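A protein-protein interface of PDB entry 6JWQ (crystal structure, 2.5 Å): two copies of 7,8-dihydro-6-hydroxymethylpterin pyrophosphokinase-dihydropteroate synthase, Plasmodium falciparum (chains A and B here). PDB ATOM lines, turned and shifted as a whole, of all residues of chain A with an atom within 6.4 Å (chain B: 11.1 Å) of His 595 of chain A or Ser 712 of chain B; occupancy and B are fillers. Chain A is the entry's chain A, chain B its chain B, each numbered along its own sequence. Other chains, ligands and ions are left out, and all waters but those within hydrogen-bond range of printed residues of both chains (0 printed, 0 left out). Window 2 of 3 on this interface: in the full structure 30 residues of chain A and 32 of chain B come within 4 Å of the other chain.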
ATOM      1  N   TYR A 549      23.162  12.319   0.219  1.00  0.00           N
ATOM      2  CA  TYR A 549      22.399  12.211  -1.028  1.00  0.00           C
ATOM      3  C   TYR A 549      22.752  10.986  -1.863  1.00  0.00           C
ATOM      4  O   TYR A 549      21.881  10.469  -2.596  1.00  0.00           O
ATOM      5  CB  TYR A 549      22.393  13.533  -1.818  1.00  0.00           C
ATOM      6  CG  TYR A 549      21.723  14.602  -1.008  1.00  0.00           C
ATOM      7  CD1 TYR A 549      20.339  14.793  -1.087  1.00  0.00           C
ATOM      8  CD2 TYR A 549      22.454  15.373  -0.080  1.00  0.00           C
ATOM      9  CE1 TYR A 549      19.699  15.749  -0.293  1.00  0.00           C
ATOM     10  CE2 TYR A 549      21.821  16.322   0.713  1.00  0.00           C
ATOM     11  CZ  TYR A 549      20.443  16.505   0.600  1.00  0.00           C
ATOM     12  OH  TYR A 549      19.806  17.455   1.389  1.00  0.00           O
ATOM     13  N   LYS A 589      26.168  11.820  10.817  1.00  0.00           N
ATOM     14  CA  LYS A 589      25.767  12.757   9.754  1.00  0.00           C
ATOM     15  C   LYS A 589      24.459  12.335   9.114  1.00  0.00           C
ATOM     16  O   LYS A 589      23.598  13.161   8.822  1.00  0.00           O
ATOM     17  CB  LYS A 589      26.845  12.857   8.680  1.00  0.00           C
ATOM     18  CG  LYS A 589      27.162  14.276   8.281  1.00  0.00           C
ATOM     19  CD  LYS A 589      26.623  14.651   6.920  1.00  0.00           C
ATOM     20  CE  LYS A 589      27.409  15.829   6.372  1.00  0.00           C
ATOM     21  NZ  LYS A 589      27.291  17.014   7.278  1.00  0.00           N
ATOM     22  N   LEU A 590      24.332  11.034   8.904  1.00  0.00           N
ATOM     23  CA  LEU A 590      23.110  10.459   8.396  1.00  0.00           C
ATOM     24  C   LEU A 590      21.913  10.768   9.311  1.00  0.00           C
ATOM     25  O   LEU A 590      20.866  11.151   8.821  1.00  0.00           O
ATOM     26  CB  LEU A 590      23.301   8.951   8.162  1.00  0.00           C
ATOM     27  CG  LEU A 590      24.116   8.601   6.908  1.00  0.00           C
ATOM     28  CD1 LEU A 590      24.465   7.115   6.906  1.00  0.00           C
ATOM     29  CD2 LEU A 590      23.424   9.004   5.612  1.00  0.00           C
ATOM     30  N   LEU A 591      22.089  10.630  10.627  1.00  0.00           N
ATOM     31  CA  LEU A 591      21.064  11.015  11.608  1.00  0.00           C
ATOM     32  C   LEU A 591      20.745  12.502  11.567  1.00  0.00           C
ATOM     33  O   LEU A 591      19.595  12.846  11.408  1.00  0.00           O
ATOM     34  CB  LEU A 591      21.446  10.586  13.028  1.00  0.00           C
ATOM     35  CG  LEU A 591      21.326   9.086  13.298  1.00  0.00           C
ATOM     36  CD1 LEU A 591      22.069   8.744  14.569  1.00  0.00           C
ATOM     37  CD2 LEU A 591      19.870   8.654  13.374  1.00  0.00           C
ATOM     38  N   GLN A 592      21.761  13.366  11.688  1.00  0.00           N
ATOM     39  CA  GLN A 592      21.594  14.829  11.592  1.00  0.00           C
ATOM     40  C   GLN A 592      20.776  15.205  10.366  1.00  0.00           C
ATOM     41  O   GLN A 592      20.050  16.180  10.394  1.00  0.00           O
ATOM     42  CB  GLN A 592      22.944  15.559  11.528  1.00  0.00           C
ATOM     43  CG  GLN A 592      23.925  15.189  12.633  1.00  0.00           C
ATOM     44  CD  GLN A 592      25.265  15.917  12.555  1.00  0.00           C
ATOM     45  OE1 GLN A 592      25.876  16.006  11.502  1.00  0.00           O
ATOM     46  NE2 GLN A 592      25.737  16.411  13.690  1.00  0.00           N
ATOM     47  N   ASN A 593      20.876  14.418   9.301  1.00  0.00           N
ATOM     48  CA  ASN A 593      20.191  14.724   8.045  1.00  0.00           C
ATOM     49  C   ASN A 593      19.032  13.814   7.697  1.00  0.00           C
ATOM     50  O   ASN A 593      18.684  13.661   6.538  1.00  0.00           O
ATOM     51  CB  ASN A 593      21.196  14.804   6.898  1.00  0.00           C
ATOM     52  CG  ASN A 593      22.130  15.952   7.066  1.00  0.00           C
ATOM     53  OD1 ASN A 593      21.811  17.084   6.706  1.00  0.00           O
ATOM     54  ND2 ASN A 593      23.278  15.680   7.659  1.00  0.00           N
ATOM     55  N   ILE A 594      18.412  13.257   8.718  1.00  0.00           N
ATOM     56  CA  ILE A 594      17.312  12.317   8.560  1.00  0.00           C
ATOM     57  C   ILE A 594      16.055  12.925   7.868  1.00  0.00           C
ATOM     58  O   ILE A 594      15.304  12.183   7.246  1.00  0.00           O
ATOM     59  CB  ILE A 594      17.043  11.598   9.925  1.00  0.00           C
ATOM     60  CG1 ILE A 594      16.528  10.182   9.754  1.00  0.00           C
ATOM     61  CG2 ILE A 594      16.134  12.395  10.821  1.00  0.00           C
ATOM     62  CD1 ILE A 594      17.576   9.214   9.273  1.00  0.00           C
ATOM     63  N   HIS A 595      15.878  14.259   7.934  1.00  0.00           N
ATOM     64  CA  HIS A 595      14.742  15.012   7.312  1.00  0.00           C
ATOM     65  C   HIS A 595      14.635  14.721   5.827  1.00  0.00           C
ATOM     66  O   HIS A 595      13.560  14.696   5.244  1.00  0.00           O
ATOM     67  CB  HIS A 595      14.877  16.535   7.526  1.00  0.00           C
ATOM     68  CG  HIS A 595      16.111  17.127   6.905  1.00  0.00           C
ATOM     69  ND1 HIS A 595      17.338  17.148   7.548  1.00  0.00           N
ATOM     70  CD2 HIS A 595      16.318  17.675   5.678  1.00  0.00           C
ATOM     71  CE1 HIS A 595      18.241  17.694   6.749  1.00  0.00           C
ATOM     72  NE2 HIS A 595      17.649  18.017   5.606  1.00  0.00           N
ATOM     73  N   VAL A 596      15.781  14.494   5.220  1.00  0.00           N
ATOM     74  CA  VAL A 596      15.903  14.050   3.829  1.00  0.00           C
ATOM     75  C   VAL A 596      14.903  12.925   3.430  1.00  0.00           C
ATOM     76  O   VAL A 596      14.544  12.797   2.260  1.00  0.00           O
ATOM     77  CB  VAL A 596      17.409  13.752   3.614  1.00  0.00           C
ATOM     78  CG1 VAL A 596      17.708  12.376   3.048  1.00  0.00           C
ATOM     79  CG2 VAL A 596      18.085  14.916   2.903  1.00  0.00           C
ATOM     80  N   TYR A 597      14.423  12.172   4.424  1.00  0.00           N
ATOM     81  CA  TYR A 597      13.431  11.098   4.246  1.00  0.00           C
ATOM     82  C   TYR A 597      12.000  11.445   4.706  1.00  0.00           C
ATOM     83  O   TYR A 597      11.182  10.527   4.936  1.00  0.00           O
ATOM     84  CB  TYR A 597      13.916   9.790   4.917  1.00  0.00           C
ATOM     85  CG  TYR A 597      15.215   9.294   4.329  1.00  0.00           C
ATOM     86  CD1 TYR A 597      15.238   8.594   3.098  1.00  0.00           C
ATOM     87  CD2 TYR A 597      16.427   9.571   4.971  1.00  0.00           C
ATOM     88  CE1 TYR A 597      16.441   8.180   2.547  1.00  0.00           C
ATOM     89  CE2 TYR A 597      17.629   9.173   4.424  1.00  0.00           C
ATOM     90  CZ  TYR A 597      17.638   8.478   3.221  1.00  0.00           C
ATOM     91  OH  TYR A 597      18.851   8.088   2.704  1.00  0.00           O
ATOM     92  N   ASP A 598      11.688  12.747   4.805  1.00  0.00           N
ATOM     93  CA  ASP A 598      10.354  13.210   5.256  1.00  0.00           C
ATOM     94  C   ASP A 598       9.221  12.734   4.365  1.00  0.00           C
ATOM     95  O   ASP A 598       8.093  12.626   4.832  1.00  0.00           O
ATOM     96  CB  ASP A 598      10.271  14.736   5.416  1.00  0.00           C
ATOM     97  CG  ASP A 598      11.054  15.259   6.634  1.00  0.00           C
ATOM     98  OD1 ASP A 598      11.472  14.469   7.511  1.00  0.00           O
ATOM     99  OD2 ASP A 598      11.277  16.485   6.709  1.00  0.00           O
ATOM    100  N   GLU A 599       9.521  12.446   3.102  1.00  0.00           N
ATOM    101  CA  GLU A 599       8.523  11.936   2.167  1.00  0.00           C
ATOM    102  C   GLU A 599       8.375  10.418   2.191  1.00  0.00           C
ATOM    103  O   GLU A 599       7.519   9.907   1.508  1.00  0.00           O
ATOM    104  CB  GLU A 599       8.869  12.323   0.713  1.00  0.00           C
ATOM    105  CG  GLU A 599       8.866  13.806   0.360  1.00  0.00           C
ATOM    106  CD  GLU A 599       7.544  14.505   0.636  1.00  0.00           C
ATOM    107  OE1 GLU A 599       6.498  14.089   0.087  1.00  0.00           O
ATOM    108  OE2 GLU A 599       7.571  15.494   1.401  1.00  0.00           O
ATOM    109  N   TYR A 676      15.140  11.323  19.542  1.00  0.00           N
ATOM    110  CA  TYR A 676      15.397  12.070  18.327  1.00  0.00           C
ATOM    111  C   TYR A 676      14.500  11.554  17.192  1.00  0.00           C
ATOM    112  O   TYR A 676      13.895  12.347  16.457  1.00  0.00           O
ATOM    113  CB  TYR A 676      16.893  11.956  17.988  1.00  0.00           C
ATOM    114  CG  TYR A 676      17.315  12.677  16.733  1.00  0.00           C
ATOM    115  CD1 TYR A 676      17.395  14.082  16.701  1.00  0.00           C
ATOM    116  CD2 TYR A 676      17.653  11.958  15.575  1.00  0.00           C
ATOM    117  CE1 TYR A 676      17.787  14.750  15.538  1.00  0.00           C
ATOM    118  CE2 TYR A 676      18.055  12.615  14.411  1.00  0.00           C
ATOM    119  CZ  TYR A 676      18.125  14.008  14.400  1.00  0.00           C
ATOM    120  OH  TYR A 676      18.516  14.666  13.259  1.00  0.00           O
ATOM    121  N   LYS A 680      11.752  13.381  14.993  1.00  0.00           N
ATOM    122  CA  LYS A 680      11.957  13.416  13.543  1.00  0.00           C
ATOM    123  C   LYS A 680      10.915  12.579  12.833  1.00  0.00           C
ATOM    124  O   LYS A 680      10.932  12.466  11.605  1.00  0.00           O
ATOM    125  CB  LYS A 680      13.380  13.041  13.155  1.00  0.00           C
ATOM    126  CG  LYS A 680      14.436  14.036  13.597  1.00  0.00           C
ATOM    127  CD  LYS A 680      14.175  15.418  13.037  1.00  0.00           C
ATOM    128  CE  LYS A 680      15.325  16.385  13.280  1.00  0.00           C
ATOM    129  NZ  LYS A 680      15.483  17.346  12.143  1.00  0.00           N
ATOM    130  N   ILE B 703      24.582  14.752  17.994  1.00  0.00           N
ATOM    131  CA  ILE B 703      23.679  14.903  16.877  1.00  0.00           C
ATOM    132  C   ILE B 703      23.531  16.387  16.517  1.00  0.00           C
ATOM    133  O   ILE B 703      23.500  16.736  15.336  1.00  0.00           O
ATOM    134  CB  ILE B 703      22.331  14.172  17.100  1.00  0.00           C
ATOM    135  CG1 ILE B 703      22.562  12.664  17.172  1.00  0.00           C
ATOM    136  CG2 ILE B 703      21.358  14.448  15.950  1.00  0.00           C
ATOM    137  CD1 ILE B 703      21.450  11.884  17.842  1.00  0.00           C
ATOM    138  N   ASP B 704      23.490  17.262  17.514  1.00  0.00           N
ATOM    139  CA  ASP B 704      23.407  18.699  17.233  1.00  0.00           C
ATOM    140  C   ASP B 704      24.707  19.355  16.740  1.00  0.00           C
ATOM    141  O   ASP B 704      24.663  20.451  16.176  1.00  0.00           O
ATOM    142  CB  ASP B 704      22.879  19.456  18.448  1.00  0.00           C
ATOM    143  CG  ASP B 704      21.384  19.386  18.577  1.00  0.00           C
ATOM    144  OD1 ASP B 704      20.685  19.005  17.607  1.00  0.00           O
ATOM    145  OD2 ASP B 704      20.889  19.714  19.672  1.00  0.00           O
ATOM    146  N   VAL B 706      27.168  20.339  14.466  1.00  0.00           N
ATOM    147  CA  VAL B 706      27.413  20.430  13.016  1.00  0.00           C
ATOM    148  C   VAL B 706      28.580  21.362  12.686  1.00  0.00           C
ATOM    149  O   VAL B 706      28.680  22.468  13.226  1.00  0.00           O
ATOM    150  CB  VAL B 706      26.147  20.826  12.200  1.00  0.00           C
ATOM    151  CG1 VAL B 706      25.158  19.666  12.132  1.00  0.00           C
ATOM    152  CG2 VAL B 706      25.476  22.089  12.751  1.00  0.00           C
ATOM    153  N   LYS B 707      29.453  20.890  11.800  1.00  0.00           N
ATOM    154  CA  LYS B 707      30.634  21.637  11.331  1.00  0.00           C
ATOM    155  C   LYS B 707      30.243  22.902  10.530  1.00  0.00           C
ATOM    156  O   LYS B 707      30.560  24.030  10.939  1.00  0.00           O
ATOM    157  CB  LYS B 707      31.556  20.720  10.496  1.00  0.00           C
ATOM    158  CG  LYS B 707      31.658  19.279  10.993  1.00  0.00           C
ATOM    159  CD  LYS B 707      32.261  18.361   9.941  1.00  0.00           C
ATOM    160  CE  LYS B 707      31.937  16.893  10.213  1.00  0.00           C
ATOM    161  NZ  LYS B 707      32.754  16.278  11.301  1.00  0.00           N
ATOM    162  N   ASP B 708      29.533  22.696   9.416  1.00  0.00           N
ATOM    163  CA  ASP B 708      29.126  23.759   8.491  1.00  0.00           C
ATOM    164  C   ASP B 708      27.587  23.941   8.473  1.00  0.00           C
ATOM    165  O   ASP B 708      26.867  23.070   7.962  1.00  0.00           O
ATOM    166  CB  ASP B 708      29.691  23.460   7.089  1.00  0.00           C
ATOM    167  CG  ASP B 708      29.407  24.558   6.071  1.00  0.00           C
ATOM    168  OD1 ASP B 708      29.221  25.740   6.451  1.00  0.00           O
ATOM    169  OD2 ASP B 708      29.391  24.228   4.867  1.00  0.00           O
ATOM    170  N   PRO B 709      27.085  25.071   9.037  1.00  0.00           N
ATOM    171  CA  PRO B 709      25.637  25.312   9.246  1.00  0.00           C
ATOM    172  C   PRO B 709      24.749  25.391   7.989  1.00  0.00           C
ATOM    173  O   PRO B 709      23.522  25.294   8.100  1.00  0.00           O
ATOM    174  CB  PRO B 709      25.600  26.646  10.015  1.00  0.00           C
ATOM    175  CG  PRO B 709      26.913  27.294   9.742  1.00  0.00           C
ATOM    176  CD  PRO B 709      27.895  26.167   9.610  1.00  0.00           C
ATOM    177  N   ASN B 710      25.356  25.571   6.819  1.00  0.00           N
ATOM    178  CA  ASN B 710      24.609  25.615   5.556  1.00  0.00           C
ATOM    179  C   ASN B 710      24.892  24.440   4.607  1.00  0.00           C
ATOM    180  O   ASN B 710      24.247  24.324   3.550  1.00  0.00           O
ATOM    181  CB  ASN B 710      24.733  26.991   4.845  1.00  0.00           C
ATOM    182  CG  ASN B 710      26.085  27.671   5.067  1.00  0.00           C
ATOM    183  OD1 ASN B 710      27.121  27.226   4.561  1.00  0.00           O
ATOM    184  ND2 ASN B 710      26.070  28.772   5.812  1.00  0.00           N
ATOM    185  N   SER B 711      25.820  23.557   5.008  1.00  0.00           N
ATOM    186  CA  SER B 711      26.186  22.355   4.229  1.00  0.00           C
ATOM    187  C   SER B 711      24.994  21.455   3.850  1.00  0.00           C
ATOM    188  O   SER B 711      25.028  20.797   2.812  1.00  0.00           O
ATOM    189  CB  SER B 711      27.306  21.547   4.907  1.00  0.00           C
ATOM    190  OG  SER B 711      26.857  20.835   6.048  1.00  0.00           O
ATOM    191  N   SER B 712      23.953  21.458   4.685  1.00  0.00           N
ATOM    192  CA  SER B 712      22.657  20.856   4.361  1.00  0.00           C
ATOM    193  C   SER B 712      22.098  21.306   2.992  1.00  0.00           C
ATOM    194  O   SER B 712      21.796  20.462   2.137  1.00  0.00           O
ATOM    195  CB  SER B 712      21.653  21.147   5.486  1.00  0.00           C
ATOM    196  OG  SER B 712      20.336  20.753   5.133  1.00  0.00           O
ATOM    197  N   SER B 713      21.974  22.624   2.792  1.00  0.00           N
ATOM    198  CA  SER B 713      21.479  23.184   1.517  1.00  0.00           C
ATOM    199  C   SER B 713      22.511  23.120   0.370  1.00  0.00           C
ATOM    200  O   SER B 713      22.137  22.983  -0.800  1.00  0.00           O
ATOM    201  CB  SER B 713      20.920  24.607   1.696  1.00  0.00           C
ATOM    202  OG  SER B 713      21.838  25.448   2.373  1.00  0.00           O
ATOM    203  N   VAL B 714      23.794  23.215   0.725  1.00  0.00           N
ATOM    204  CA  VAL B 714      24.917  23.082  -0.213  1.00  0.00           C
ATOM    205  C   VAL B 714      24.979  21.671  -0.833  1.00  0.00           C
ATOM    206  O   VAL B 714      25.022  21.544  -2.066  1.00  0.00           O
ATOM    207  CB  VAL B 714      26.260  23.481   0.460  1.00  0.00           C
ATOM    208  CG1 VAL B 714      27.454  23.163  -0.423  1.00  0.00           C
ATOM    209  CG2 VAL B 714      26.259  24.957   0.808  1.00  0.00           C
ATOM    210  N   ASP B 715      24.970  20.631   0.016  1.00  0.00           N
ATOM    211  CA  ASP B 715      24.934  19.225  -0.431  1.00  0.00           C
ATOM    212  C   ASP B 715      23.669  18.904  -1.234  1.00  0.00           C
ATOM    213  O   ASP B 715      23.744  18.194  -2.250  1.00  0.00           O
ATOM    214  CB  ASP B 715      25.084  18.262   0.752  1.00  0.00           C
ATOM    215  CG  ASP B 715      26.442  18.390   1.455  1.00  0.00           C
ATOM    216  OD1 ASP B 715      27.390  18.906   0.820  1.00  0.00           O
ATOM    217  OD2 ASP B 715      26.574  17.977   2.639  1.00  0.00           O
ATOM    218  N   LYS B 716      22.528  19.446  -0.783  1.00  0.00           N
ATOM    219  CA  LYS B 716      21.251  19.288  -1.472  1.00  0.00           C
ATOM    220  C   LYS B 716      21.368  19.813  -2.894  1.00  0.00           C
ATOM    221  O   LYS B 716      20.957  19.124  -3.844  1.00  0.00           O
ATOM    222  CB  LYS B 716      20.077  19.967  -0.718  1.00  0.00           C
ATOM    223  CG  LYS B 716      18.704  19.683  -1.362  1.00  0.00           C
ATOM    224  CD  LYS B 716      17.524  19.735  -0.398  1.00  0.00           C
ATOM    225  CE  LYS B 716      16.830  21.087  -0.410  1.00  0.00           C
ATOM    226  NZ  LYS B 716      16.184  21.409   0.897  1.00  0.00           N
ATOM    227  N   LEU B 717      21.945  21.017  -3.023  1.00  0.00           N
ATOM    228  CA  LEU B 717      22.148  21.682  -4.320  1.00  0.00           C
ATOM    229  C   LEU B 717      23.076  20.888  -5.242  1.00  0.00           C
ATOM    230  O   LEU B 717      22.750  20.703  -6.420  1.00  0.00           O
ATOM    231  CB  LEU B 717      22.634  23.132  -4.146  1.00  0.00           C
ATOM    232  CG  LEU B 717      22.793  24.013  -5.398  1.00  0.00           C
ATOM    233  CD1 LEU B 717      21.488  24.218  -6.154  1.00  0.00           C
ATOM    234  CD2 LEU B 717      23.395  25.357  -5.020  1.00  0.00           C
ATOM    235  N   ALA B 718      24.198  20.410  -4.690  1.00  0.00           N
ATOM    236  CA  ALA B 718      25.144  19.552  -5.406  1.00  0.00           C
ATOM    237  C   ALA B 718      24.459  18.301  -5.966  1.00  0.00           C
ATOM    238  O   ALA B 718      24.723  17.921  -7.117  1.00  0.00           O
ATOM    239  CB  ALA B 718      26.330  19.168  -4.518  1.00  0.00           C
ATOM    240  N   ALA B 719      23.574  17.688  -5.165  1.00  0.00           N
ATOM    241  CA  ALA B 719      22.774  16.536  -5.606  1.00  0.00           C
ATOM    242  C   ALA B 719      21.824  16.885  -6.754  1.00  0.00           C
ATOM    243  O   ALA B 719      21.690  16.122  -7.716  1.00  0.00           O
ATOM    244  CB  ALA B 719      22.000  15.950  -4.439  1.00  0.00           C
ATOM    245  N   ALA B 720      21.171  18.039  -6.637  1.00  0.00           N
ATOM    246  CA  ALA B 720      20.273  18.532  -7.665  1.00  0.00           C
ATOM    247  C   ALA B 720      20.988  18.789  -9.009  1.00  0.00           C
ATOM    248  O   ALA B 720      20.406  18.558 -10.069  1.00  0.00           O
ATOM    249  CB  ALA B 720      19.555  19.781  -7.171  1.00  0.00           C
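Of chain B, only Ser 712 comes within 4 Å of His 595 of chain A. Printed residues of chain A within 4 Å of Ser 712 of chain B: Tyr 549 and His 595. No residue of chain B comes within 4 Å of Ile 594 of chain A. Val 596 of chain A touches none of the printed residues of chain B. Asp 598 of chain A touches none of the printed residues of chain B. Of the printed residues of chain A, Ala 719 of chain B touches Tyr 549. Printed residues of chain A within 4 Å of Val 706 of chain B: Gln 592. Lys 680 of chain A touches none of the printed residues of chain B. Leu 590 of chain A touches none of the printed residues of chain B. The nearest residue of chain B that does not touch His 595 of chain A is Lys 716 of chain B (6.0 Å). The nearest residue of chain A that does not touch Ser 712 of chain B is Asn 593 of chain A (4.2 Å). The nearest printed residue of chain A that does not touch Ala 719 of chain B is Val 596 of chain A (8.4 Å).
Among the printed residues, merely in contact across the chains: Tyr 549 of chain A with Ser 712 of chain B (3.7 Å), Tyr 549 of chain A with Asp 715 of chain B (3.7 Å), Tyr 549 of chain A with Lys 716 of chain B (3.3 Å), Tyr 549 of chain A with Ala 719 of chain B (3.6 Å), Gln 592 of chain A with Val 706 of chain B (3.7 Å), His 595 of chain A with Ser 712 of chain B (3.9 Å) and Tyr 676 of chain A with Ile 703 of chain B (3.6 Å).
No position is printed for both chains.
Printed residues of chain A that touch a printed residue of chain B: Tyr 549, Gln 592, His 595 and Tyr 676. Hydrophobic or aromatic side chains of chain A within 4 Å of the printed part of chain B: Tyr 549, His 595 and Tyr 676. Of the 17 printed residues of chain B, 6 touch a printed residue of chain A. Printed residues of chain B that touch a printed residue of chain A: Ile 703, Val 706, Ser 712, Asp 715, Lys 716 and Ala 719. Hydrophobic or aromatic side chains of chain B that line the printed part of chain A: Ile 703, Val 706 and Ala 719. Among the printed residues, 8 pairs touch across the chains.
The backbone carbonyl oxygen of Leu 591 of chain A is in hydrogen-bond range of the side-chain hydroxyl of Tyr 676 of chain A (2.8 Å).
The side-chain amide nitrogen (NE2) of Gln 592 of chain A is in hydrogen-bond range of the backbone carbonyl oxygen (O) of Ile 703 of chain B (2.8 Å).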
